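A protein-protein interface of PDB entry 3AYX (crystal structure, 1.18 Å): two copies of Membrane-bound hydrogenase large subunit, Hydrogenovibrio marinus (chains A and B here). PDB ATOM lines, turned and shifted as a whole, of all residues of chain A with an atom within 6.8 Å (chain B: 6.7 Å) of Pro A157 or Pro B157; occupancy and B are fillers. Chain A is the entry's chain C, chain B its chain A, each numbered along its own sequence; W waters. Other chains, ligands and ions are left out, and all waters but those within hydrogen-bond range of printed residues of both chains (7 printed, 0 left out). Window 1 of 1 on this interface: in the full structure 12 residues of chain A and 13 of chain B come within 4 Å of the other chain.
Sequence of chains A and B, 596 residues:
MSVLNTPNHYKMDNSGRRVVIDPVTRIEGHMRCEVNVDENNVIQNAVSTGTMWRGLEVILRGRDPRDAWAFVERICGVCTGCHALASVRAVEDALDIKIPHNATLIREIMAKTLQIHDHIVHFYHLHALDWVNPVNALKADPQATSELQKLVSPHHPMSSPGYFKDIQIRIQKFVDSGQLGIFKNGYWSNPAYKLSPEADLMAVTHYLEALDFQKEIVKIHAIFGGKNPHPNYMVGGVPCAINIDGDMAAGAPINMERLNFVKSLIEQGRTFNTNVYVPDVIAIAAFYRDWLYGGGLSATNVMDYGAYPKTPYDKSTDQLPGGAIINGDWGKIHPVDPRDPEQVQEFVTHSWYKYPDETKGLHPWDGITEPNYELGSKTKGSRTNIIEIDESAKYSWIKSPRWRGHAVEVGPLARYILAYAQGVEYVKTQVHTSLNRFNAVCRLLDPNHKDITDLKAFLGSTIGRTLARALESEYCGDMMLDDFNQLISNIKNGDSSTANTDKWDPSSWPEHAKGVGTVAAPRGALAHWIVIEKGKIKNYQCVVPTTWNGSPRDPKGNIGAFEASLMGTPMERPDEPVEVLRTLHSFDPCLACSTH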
ATOM      1  N   GLN A 149     -30.229 -19.857  31.306  1.00  0.00           N
ATOM      2  CA  GLN A 149     -29.809 -20.240  29.961  1.00  0.00           C
ATOM      3  C   GLN A 149     -28.323 -20.563  30.007  1.00  0.00           C
ATOM      4  O   GLN A 149     -27.912 -21.568  29.433  1.00  0.00           O
ATOM      5  CB  GLN A 149     -30.014 -19.129  28.997  1.00  0.00           C
ATOM      6  CG  GLN A 149     -29.446 -19.268  27.594  1.00  0.00           C
ATOM      7  CD  GLN A 149     -29.989 -20.419  26.808  1.00  0.00           C
ATOM      8  OE1 GLN A 149     -31.171 -20.547  26.635  1.00  0.00           O
ATOM      9  NE2 GLN A 149     -29.140 -21.298  26.368  1.00  0.00           N
ATOM     10  N   SER A 153     -27.076 -24.450  29.044  1.00  0.00           N
ATOM     11  CA  SER A 153     -26.315 -24.672  27.824  1.00  0.00           C
ATOM     12  C   SER A 153     -25.282 -23.565  27.653  1.00  0.00           C
ATOM     13  O   SER A 153     -25.529 -22.605  26.935  1.00  0.00           O
ATOM     14  CB  SER A 153     -27.229 -24.669  26.616  1.00  0.00           C
ATOM     15  OG  SER A 153     -26.429 -25.140  25.528  1.00  0.00           O
ATOM     16  N   PRO A 154     -24.160 -23.700  28.287  1.00  0.00           N
ATOM     17  CA  PRO A 154     -23.182 -22.600  28.243  1.00  0.00           C
ATOM     18  C   PRO A 154     -22.683 -22.246  26.878  1.00  0.00           C
ATOM     19  O   PRO A 154     -22.303 -21.105  26.652  1.00  0.00           O
ATOM     20  CB  PRO A 154     -22.065 -23.144  29.137  1.00  0.00           C
ATOM     21  CG  PRO A 154     -22.478 -24.373  29.759  1.00  0.00           C
ATOM     22  CD  PRO A 154     -23.771 -24.834  29.156  1.00  0.00           C
ATOM     23  N   HIS A 155     -22.642 -23.141  25.894  1.00  0.00           N
ATOM     24  CA  HIS A 155     -22.141 -22.842  24.583  1.00  0.00           C
ATOM     25  C   HIS A 155     -23.162 -22.155  23.684  1.00  0.00           C
ATOM     26  O   HIS A 155     -22.789 -21.569  22.654  1.00  0.00           O
ATOM     27  CB  HIS A 155     -21.691 -24.106  23.862  1.00  0.00           C
ATOM     28  CG  HIS A 155     -20.479 -24.716  24.481  1.00  0.00           C
ATOM     29  ND1 HIS A 155     -19.205 -24.312  24.226  1.00  0.00           N
ATOM     30  CD2 HIS A 155     -20.373 -25.709  25.398  1.00  0.00           C
ATOM     31  CE1 HIS A 155     -18.369 -25.042  24.936  1.00  0.00           C
ATOM     32  NE2 HIS A 155     -19.059 -25.922  25.668  1.00  0.00           N
ATOM     33  N   HIS A 156     -24.430 -22.251  24.041  1.00  0.00           N
ATOM     34  CA  HIS A 156     -25.403 -21.624  23.135  1.00  0.00           C
ATOM     35  C   HIS A 156     -25.222 -20.105  23.121  1.00  0.00           C
ATOM     36  O   HIS A 156     -25.256 -19.518  24.220  1.00  0.00           O
ATOM     37  CB  HIS A 156     -26.848 -21.985  23.506  1.00  0.00           C
ATOM     38  CG  HIS A 156     -27.842 -21.569  22.488  1.00  0.00           C
ATOM     39  ND1 HIS A 156     -27.712 -21.756  21.140  1.00  0.00           N
ATOM     40  CD2 HIS A 156     -29.080 -21.028  22.688  1.00  0.00           C
ATOM     41  CE1 HIS A 156     -28.785 -21.369  20.514  1.00  0.00           C
ATOM     42  NE2 HIS A 156     -29.631 -20.895  21.409  1.00  0.00           N
ATOM     43  N   PRO A 157     -25.016 -19.464  21.991  1.00  0.00           N
ATOM     44  CA  PRO A 157     -24.760 -18.034  22.060  1.00  0.00           C
ATOM     45  C   PRO A 157     -25.900 -17.131  22.493  1.00  0.00           C
ATOM     46  O   PRO A 157     -25.661 -16.007  22.947  1.00  0.00           O
ATOM     47  CB  PRO A 157     -24.320 -17.653  20.598  1.00  0.00           C
ATOM     48  CG  PRO A 157     -23.820 -18.938  20.078  1.00  0.00           C
ATOM     49  CD  PRO A 157     -24.779 -19.989  20.660  1.00  0.00           C
ATOM     50  N   MET A 158     -27.155 -17.567  22.322  1.00  0.00           N
ATOM     51  CA  MET A 158     -28.369 -16.742  22.378  1.00  0.00           C
ATOM     52  C   MET A 158     -28.858 -16.589  23.811  1.00  0.00           C
ATOM     53  O   MET A 158     -29.808 -17.225  24.228  1.00  0.00           O
ATOM     54  CB  MET A 158     -29.483 -17.280  21.492  1.00  0.00           C
ATOM     55  CG  MET A 158     -29.105 -17.642  20.066  1.00  0.00           C
ATOM     56  SD  MET A 158     -28.981 -16.155  19.063  1.00  0.00           S
ATOM     57  CE  MET A 158     -30.699 -15.798  18.940  1.00  0.00           C
ATOM     58  N   SER A 159     -28.195 -15.797  24.629  1.00  0.00           N
ATOM     59  CA  SER A 159     -28.548 -15.735  26.020  1.00  0.00           C
ATOM     60  C   SER A 159     -28.752 -14.350  26.559  1.00  0.00           C
ATOM     61  O   SER A 159     -28.958 -14.200  27.754  1.00  0.00           O
ATOM     62  CB  SER A 159     -27.436 -16.426  26.832  1.00  0.00           C
ATOM     63  OG  SER A 159     -26.224 -15.706  26.830  1.00  0.00           O
ATOM     64  N   SER A 160     -28.663 -13.265  25.775  1.00  0.00           N
ATOM     65  CA  SER A 160     -28.740 -11.927  26.332  1.00  0.00           C
ATOM     66  C   SER A 160     -30.021 -11.708  27.112  1.00  0.00           C
ATOM     67  O   SER A 160     -31.075 -12.063  26.604  1.00  0.00           O
ATOM     68  CB  SER A 160     -28.710 -10.858  25.213  1.00  0.00           C
ATOM     69  OG  SER A 160     -27.502 -11.095  24.519  1.00  0.00           O
ATOM     70  N   PRO A 161     -29.914 -11.043  28.274  1.00  0.00           N
ATOM     71  CA  PRO A 161     -31.162 -10.634  28.954  1.00  0.00           C
ATOM     72  C   PRO A 161     -32.081  -9.874  28.021  1.00  0.00           C
ATOM     73  O   PRO A 161     -33.256 -10.052  28.055  1.00  0.00           O
ATOM     74  CB  PRO A 161     -30.668  -9.757  30.139  1.00  0.00           C
ATOM     75  CG  PRO A 161     -29.277 -10.197  30.386  1.00  0.00           C
ATOM     76  CD  PRO A 161     -28.734 -10.647  29.034  1.00  0.00           C
ATOM     77  N   GLY A 162     -31.502  -8.974  27.197  1.00  0.00           N
ATOM     78  CA  GLY A 162     -32.303  -8.168  26.315  1.00  0.00           C
ATOM     79  C   GLY A 162     -33.022  -8.951  25.255  1.00  0.00           C
ATOM     80  O   GLY A 162     -34.121  -8.612  24.832  1.00  0.00           O
ATOM     81  N   TYR A 163     -32.408 -10.055  24.816  1.00  0.00           N
ATOM     82  CA  TYR A 163     -33.074 -10.999  23.905  1.00  0.00           C
ATOM     83  C   TYR A 163     -34.255 -11.656  24.576  1.00  0.00           C
ATOM     84  O   TYR A 163     -35.338 -11.677  23.994  1.00  0.00           O
ATOM     85  CB  TYR A 163     -32.080 -12.006  23.448  1.00  0.00           C
ATOM     86  CG  TYR A 163     -32.602 -13.206  22.665  1.00  0.00           C
ATOM     87  CD1 TYR A 163     -33.329 -13.045  21.515  1.00  0.00           C
ATOM     88  CD2 TYR A 163     -32.320 -14.492  23.073  1.00  0.00           C
ATOM     89  CE1 TYR A 163     -33.812 -14.133  20.735  1.00  0.00           C
ATOM     90  CE2 TYR A 163     -32.767 -15.576  22.329  1.00  0.00           C
ATOM     91  CZ  TYR A 163     -33.520 -15.385  21.187  1.00  0.00           C
ATOM     92  OH  TYR A 163     -33.948 -16.480  20.441  1.00  0.00           O
ATOM     93  N   ASP A 166     -37.007  -9.115  24.868  1.00  0.00           N
ATOM     94  CA  ASP A 166     -37.640  -8.892  23.590  1.00  0.00           C
ATOM     95  C   ASP A 166     -38.619 -10.002  23.231  1.00  0.00           C
ATOM     96  O   ASP A 166     -39.725  -9.746  22.699  1.00  0.00           O
ATOM     97  CB  ASP A 166     -36.543  -8.711  22.507  1.00  0.00           C
ATOM     98  CG  ASP A 166     -35.845  -7.377  22.560  1.00  0.00           C
ATOM     99  OD1 ASP A 166     -36.368  -6.448  23.257  1.00  0.00           O
ATOM    100  OD2 ASP A 166     -34.782  -7.238  21.923  1.00  0.00           O
ATOM    101  N   GLU A 209     -36.882 -20.592  18.294  1.00  0.00           N
ATOM    102  CA  GLU A 209     -35.621 -20.911  17.636  1.00  0.00           C
ATOM    103  C   GLU A 209     -35.767 -22.215  16.895  1.00  0.00           C
ATOM    104  O   GLU A 209     -35.206 -22.344  15.771  1.00  0.00           O
ATOM    105  CB  GLU A 209     -34.441 -20.980  18.621  1.00  0.00           C
ATOM    106  CG  GLU A 209     -34.056 -19.609  19.201  1.00  0.00           C
ATOM    107  CD  GLU A 209     -32.941 -19.653  20.198  1.00  0.00           C
ATOM    108  OE1 GLU A 209     -32.072 -20.576  20.075  1.00  0.00           O
ATOM    109  OE2 GLU A 209     -32.888 -18.766  21.085  1.00  0.00           O
ATOM    110  N   THR A 271     -25.093 -28.929  15.868  1.00  0.00           N
ATOM    111  CA  THR A 271     -24.990 -27.843  16.814  1.00  0.00           C
ATOM    112  C   THR A 271     -26.333 -27.598  17.518  1.00  0.00           C
ATOM    113  O   THR A 271     -26.342 -27.372  18.760  1.00  0.00           O
ATOM    114  CB  THR A 271     -24.513 -26.585  16.080  1.00  0.00           C
ATOM    115  OG1 THR A 271     -23.187 -26.844  15.592  1.00  0.00           O
ATOM    116  CG2 THR A 271     -24.463 -25.434  17.055  1.00  0.00           C
ATOM    117  N   ASN A 275     -26.540 -27.938  21.487  1.00  0.00           N
ATOM    118  CA  ASN A 275     -26.603 -26.649  22.213  1.00  0.00           C
ATOM    119  C   ASN A 275     -28.004 -26.255  22.645  1.00  0.00           C
ATOM    120  O   ASN A 275     -28.114 -25.386  23.496  1.00  0.00           O
ATOM    121  CB  ASN A 275     -26.026 -25.509  21.408  1.00  0.00           C
ATOM    122  CG  ASN A 275     -24.507 -25.540  21.307  1.00  0.00           C
ATOM    123  OD1 ASN A 275     -23.848 -26.387  21.932  1.00  0.00           O
ATOM    124  ND2 ASN A 275     -23.990 -24.655  20.486  1.00  0.00           N
ATOM    125  N   GLN B 149     -20.332  -6.706  26.071  1.00  0.00           N
ATOM    126  CA  GLN B 149     -21.277  -6.910  24.983  1.00  0.00           C
ATOM    127  C   GLN B 149     -22.640  -6.474  25.388  1.00  0.00           C
ATOM    128  O   GLN B 149     -23.334  -5.781  24.635  1.00  0.00           O
ATOM    129  CB  GLN B 149     -21.271  -8.383  24.598  1.00  0.00           C
ATOM    130  CG  GLN B 149     -22.342  -8.824  23.634  1.00  0.00           C
ATOM    131  CD  GLN B 149     -22.206  -8.196  22.273  1.00  0.00           C
ATOM    132  OE1 GLN B 149     -21.181  -8.189  21.675  1.00  0.00           O
ATOM    133  NE2 GLN B 149     -23.318  -7.709  21.805  1.00  0.00           N
ATOM    134  N   SER B 153     -24.497  -3.378  23.395  1.00  0.00           N
ATOM    135  CA  SER B 153     -25.671  -3.592  22.556  1.00  0.00           C
ATOM    136  C   SER B 153     -26.604  -4.528  23.304  1.00  0.00           C
ATOM    137  O   SER B 153     -26.566  -5.750  23.077  1.00  0.00           O
ATOM    138  CB  SER B 153     -25.331  -4.172  21.201  1.00  0.00           C
ATOM    139  OG  SER B 153     -26.520  -4.211  20.411  1.00  0.00           O
ATOM    140  N   PRO B 154     -27.451  -4.029  24.184  1.00  0.00           N
ATOM    141  CA  PRO B 154     -28.274  -4.910  25.003  1.00  0.00           C
ATOM    142  C   PRO B 154     -29.206  -5.812  24.222  1.00  0.00           C
ATOM    143  O   PRO B 154     -29.584  -6.879  24.700  1.00  0.00           O
ATOM    144  CB  PRO B 154     -29.106  -3.952  25.861  1.00  0.00           C
ATOM    145  CG  PRO B 154     -28.414  -2.629  25.824  1.00  0.00           C
ATOM    146  CD  PRO B 154     -27.574  -2.610  24.587  1.00  0.00           C
ATOM    147  N   HIS B 155     -29.686  -5.443  23.040  1.00  0.00           N
ATOM    148  CA  HIS B 155     -30.625  -6.239  22.302  1.00  0.00           C
ATOM    149  C   HIS B 155     -29.953  -7.364  21.527  1.00  0.00           C
ATOM    150  O   HIS B 155     -30.637  -8.292  21.096  1.00  0.00           O
ATOM    151  CB  HIS B 155     -31.444  -5.377  21.345  1.00  0.00           C
ATOM    152  CG  HIS B 155     -32.364  -4.441  22.025  1.00  0.00           C
ATOM    153  ND1 HIS B 155     -33.610  -4.834  22.441  1.00  0.00           N
ATOM    154  CD2 HIS B 155     -32.201  -3.141  22.356  1.00  0.00           C
ATOM    155  CE1 HIS B 155     -34.185  -3.818  23.027  1.00  0.00           C
ATOM    156  NE2 HIS B 155     -33.374  -2.778  22.961  1.00  0.00           N
ATOM    157  N   HIS B 156     -28.652  -7.288  21.249  1.00  0.00           N
ATOM    158  CA  HIS B 156     -28.069  -8.335  20.424  1.00  0.00           C
ATOM    159  C   HIS B 156     -28.078  -9.654  21.181  1.00  0.00           C
ATOM    160  O   HIS B 156     -27.614  -9.690  22.314  1.00  0.00           O
ATOM    161  CB  HIS B 156     -26.655  -7.975  20.052  1.00  0.00           C
ATOM    162  CG  HIS B 156     -26.071  -8.890  19.025  1.00  0.00           C
ATOM    163  ND1 HIS B 156     -26.758  -9.317  17.891  1.00  0.00           N
ATOM    164  CD2 HIS B 156     -24.833  -9.451  18.883  1.00  0.00           C
ATOM    165  CE1 HIS B 156     -25.949 -10.055  17.167  1.00  0.00           C
ATOM    166  NE2 HIS B 156     -24.790 -10.156  17.743  1.00  0.00           N
ATOM    167  N   PRO B 157     -28.638 -10.718  20.661  1.00  0.00           N
ATOM    168  CA  PRO B 157     -28.725 -11.953  21.462  1.00  0.00           C
ATOM    169  C   PRO B 157     -27.422 -12.653  21.808  1.00  0.00           C
ATOM    170  O   PRO B 157     -27.399 -13.386  22.789  1.00  0.00           O
ATOM    171  CB  PRO B 157     -29.588 -12.893  20.588  1.00  0.00           C
ATOM    172  CG  PRO B 157     -30.433 -11.913  19.795  1.00  0.00           C
ATOM    173  CD  PRO B 157     -29.449 -10.845  19.415  1.00  0.00           C
ATOM    174  N   MET B 158     -26.405 -12.448  20.985  1.00  0.00           N
ATOM    175  CA  MET B 158     -25.203 -13.254  20.927  1.00  0.00           C
ATOM    176  C   MET B 158     -24.173 -12.823  21.973  1.00  0.00           C
ATOM    177  O   MET B 158     -23.176 -12.204  21.635  1.00  0.00           O
ATOM    178  CB  MET B 158     -24.553 -13.226  19.548  1.00  0.00           C
ATOM    179  CG  MET B 158     -25.404 -13.550  18.358  1.00  0.00           C
ATOM    180  SD  MET B 158     -25.820 -15.324  18.237  1.00  0.00           S
ATOM    181  CE  MET B 158     -24.185 -15.872  17.711  1.00  0.00           C
ATOM    182  N   SER B 159     -24.427 -13.054  23.263  1.00  0.00           N
ATOM    183  CA  SER B 159     -23.555 -12.532  24.281  1.00  0.00           C
ATOM    184  C   SER B 159     -23.018 -13.545  25.247  1.00  0.00           C
ATOM    185  O   SER B 159     -22.321 -13.212  26.204  1.00  0.00           O
ATOM    186  CB  SER B 159     -24.323 -11.460  25.061  1.00  0.00           C
ATOM    187  OG  SER B 159     -25.391 -12.016  25.780  1.00  0.00           O
ATOM    188  N   SER B 160     -23.308 -14.856  25.095  1.00  0.00           N
ATOM    189  CA  SER B 160     -22.909 -15.841  26.072  1.00  0.00           C
ATOM    190  C   SER B 160     -21.409 -15.847  26.329  1.00  0.00           C
ATOM    191  O   SER B 160     -20.633 -15.823  25.385  1.00  0.00           O
ATOM    192  CB  SER B 160     -23.279 -17.254  25.582  1.00  0.00           C
ATOM    193  OG  SER B 160     -24.693 -17.287  25.385  1.00  0.00           O
ATOM    194  N   PRO B 161     -20.994 -15.921  27.589  1.00  0.00           N
ATOM    195  CA  PRO B 161     -19.548 -16.096  27.871  1.00  0.00           C
ATOM    196  C   PRO B 161     -18.952 -17.276  27.119  1.00  0.00           C
ATOM    197  O   PRO B 161     -17.850 -17.221  26.610  1.00  0.00           O
ATOM    198  CB  PRO B 161     -19.485 -16.265  29.367  1.00  0.00           C
ATOM    199  CG  PRO B 161     -20.736 -15.630  29.911  1.00  0.00           C
ATOM    200  CD  PRO B 161     -21.738 -15.772  28.833  1.00  0.00           C
ATOM    201  N   GLY B 162     -19.724 -18.340  27.069  1.00  0.00           N
ATOM    202  CA  GLY B 162     -19.219 -19.528  26.365  1.00  0.00           C
ATOM    203  C   GLY B 162     -19.034 -19.376  24.879  1.00  0.00           C
ATOM    204  O   GLY B 162     -18.173 -20.010  24.270  1.00  0.00           O
ATOM    205  N   TYR B 163     -19.904 -18.544  24.275  1.00  0.00           N
ATOM    206  CA  TYR B 163     -19.718 -18.176  22.881  1.00  0.00           C
ATOM    207  C   TYR B 163     -18.443 -17.386  22.678  1.00  0.00           C
ATOM    208  O   TYR B 163     -17.647 -17.736  21.820  1.00  0.00           O
ATOM    209  CB  TYR B 163     -20.910 -17.346  22.448  1.00  0.00           C
ATOM    210  CG  TYR B 163     -20.823 -16.719  21.082  1.00  0.00           C
ATOM    211  CD1 TYR B 163     -20.561 -17.422  19.946  1.00  0.00           C
ATOM    212  CD2 TYR B 163     -21.083 -15.328  20.945  1.00  0.00           C
ATOM    213  CE1 TYR B 163     -20.511 -16.826  18.690  1.00  0.00           C
ATOM    214  CE2 TYR B 163     -21.056 -14.711  19.689  1.00  0.00           C
ATOM    215  CZ  TYR B 163     -20.781 -15.464  18.568  1.00  0.00           C
ATOM    216  OH  TYR B 163     -20.712 -14.897  17.313  1.00  0.00           O
ATOM    217  N   THR B 271     -31.822  -5.036  11.435  1.00  0.00           N
ATOM    218  CA  THR B 271     -31.445  -5.562  12.725  1.00  0.00           C
ATOM    219  C   THR B 271     -29.966  -5.563  12.900  1.00  0.00           C
ATOM    220  O   THR B 271     -29.437  -5.253  13.953  1.00  0.00           O
ATOM    221  CB  THR B 271     -32.068  -7.008  12.866  1.00  0.00           C
ATOM    222  OG1 THR B 271     -33.475  -6.868  12.824  1.00  0.00           O
ATOM    223  CG2 THR B 271     -31.654  -7.600  14.181  1.00  0.00           C
ATOM    224  N   ASN B 275     -28.246  -3.567  15.894  1.00  0.00           N
ATOM    225  CA  ASN B 275     -27.801  -4.381  17.015  1.00  0.00           C
ATOM    226  C   ASN B 275     -26.329  -4.685  16.989  1.00  0.00           C
ATOM    227  O   ASN B 275     -25.803  -5.079  18.054  1.00  0.00           O
ATOM    228  CB  ASN B 275     -28.532  -5.751  17.036  1.00  0.00           C
ATOM    229  CG  ASN B 275     -29.979  -5.571  17.517  1.00  0.00           C
ATOM    230  OD1 ASN B 275     -30.449  -4.482  17.876  1.00  0.00           O
ATOM    231  ND2 ASN B 275     -30.674  -6.687  17.493  1.00  0.00           N
HETATM  232  O   HOH W   1     -33.231  -9.192  20.925  1.00  0.00           O
HETATM  233  O   HOH W   2     -35.055  -5.874  19.452  1.00  0.00           O
HETATM  234  O   HOH W   3     -28.748  -7.881  27.115  1.00  0.00           O
HETATM  235  O   HOH W   4     -26.073 -19.922  26.861  1.00  0.00           O
HETATM  236  O   HOH W   5     -25.720  -8.260  23.861  1.00  0.00           O
HETATM  237  O   HOH W   6     -22.113 -19.112  28.518  1.00  0.00           O
HETATM  238  O   HOH W   7     -25.331 -13.436  28.281  1.00  0.00           O
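The side-chain hydroxyl of Ser A160 sits at hydrogen-bond distance from the backbone carbonyl oxygen of Pro B157 (2.9 Å).
The side-chain hydroxyl of Ser B160 sits at hydrogen-bond distance from the side-chain hydroxyl of Ser A159 (2.6 Å).
The side-chain hydroxyl (OG) of Ser B160 lies within hydrogen-bond range of the backbone carbonyl oxygen (O) of Pro A157, at 2.9 Å.
ND1 of His B155 is in hydrogen-bond range of OD2 of Asp A166 (2.7 Å).
The side-chain hydroxyl (OG) of Ser B160 lies within hydrogen-bond range of the backbone carbonyl oxygen (O) of His A156, 2.6 Å away.
SD of Met B158 sits close to SD of Met A158 (3.4 Å).
The backbone carbonyl oxygen (O) of His B156 is in hydrogen-bond range of the side-chain hydroxyl (OG) of Ser A160 (2.6 Å).
The backbone carbonyl oxygen of Pro A157 sits close to the backbone carbonyl oxygen of Pro B157, 3.1 Å away.
N of Ser B159 lies within hydrogen-bond range of O of Pro A157, 3.2 Å away.
The backbone carbonyl oxygen of Pro B157 sits at hydrogen-bond distance from the backbone NH of Ser A159 (3.1 Å).
The side-chain hydroxyl of Ser B159 lies within hydrogen-bond range of the side-chain hydroxyl of Ser A160 (2.6 Å).
OE1 of Glu A209 sits at hydrogen-bond distance from NE2 of His A156.
OH of Tyr A163 is in hydrogen-bond range of OE2 of Glu A209, at 2.6 Å.
Gly B162 touches Pro A154 (CA to O, 3.5 Å).
Met B158 touches Pro A157 (CE to CB, 3.4 Å).
Pro A157 touches Tyr B163 (CG to CD1, 3.6 Å).
CA of Met A158 touches O of Pro B157, 3.5 Å away.
Ser B160 touches Met A158.
Ser A159 touches Ser B159.
Met B158 touches Ser A160 (N to OG, 3.9 Å).
Pro B154 touches Gly A162 (O to CA, 3.4 Å).
Tyr A163 touches Pro B157.
Printed residues of chain B within 4 Å of Pro A154: Gly B162 (3.5 Å).
Of the printed residues of chain B, Pro A157 touches Pro B157, Met B158, Ser B159, Ser B160 and Tyr B163.
Of the printed residues of chain B, Ser A159 touches Pro B157 (3.1 Å), Ser B159 (3.9 Å) and Ser B160 (2.6 Å).
Of the printed residues of chain B, Asp A166 touches His B155.
Asn A275 touches none of the printed residues of chain B.
Printed residues of chain A within 4 Å of Pro B157: Pro A157, Met A158, Ser A159, Ser A160 and Tyr A163.
The nearest printed residue of chain B that does not touch Pro A157 is Gly B162 (6.5 Å).
The nearest printed residue of chain A that does not touch Pro B157 is Gly A162 (6.5 Å).
The nearest printed residue of chain A that does not touch Met B158 is Ser A159 (5.3 Å).
Hydrophobic or aromatic side chains of chain A within 4 Å of the printed part of chain B: Pro A157, Met A158 and Tyr A163.
Of the 14 printed residues of chain B, 9 touch a printed residue of chain A.
Among the printed residues, 20 pairs touch across the chains.
Among the printed residues, no Asp or Glu carboxylate lies within 4 Å of a Lys or Arg side-chain nitrogen of the other chain.
Pro A154 touches Gly B162, and with the chains exchanged Gly A162 touches Pro B154.
Pro A157 touches Ser B159, and with the chains exchanged Ser A159 touches Pro B157.
Pro A157 touches Tyr B163, and with the chains exchanged Tyr A163 touches Pro B157.
Ser A159 touches its own counterpart, Ser B159.
Water W1 bridges the side-chain carboxylate (OD2) of Asp A166 and the backbone carbonyl oxygen (O) of His B155.
Water W6 bridges the backbone carbonyl oxygen of Pro A154 (2.7 Å) and the backbone NH of Gly B162 (2.9 Å).
Water W4 lies within hydrogen-bond range of O of Ser A153 (2.7 Å), O of His A156 (2.8 Å), OG of Ser B160 (3.3 Å) and NE2 of Gln A149 (3.4 Å).
Water W3 bridges the backbone carbonyl oxygen (O) of Pro B154 (2.7 Å) and the backbone NH (N) of Gly A162 (3.0 Å).
Water W2 bridges the side-chain carboxylate of Asp A166 (2.8 Å) and a ring nitrogen (ND1) of His B155 (3.5 Å).
Water W7 bridges the side-chain hydroxyl of Ser A159 (2.8 Å) and the side-chain hydroxyl of Ser B159 (2.9 Å).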
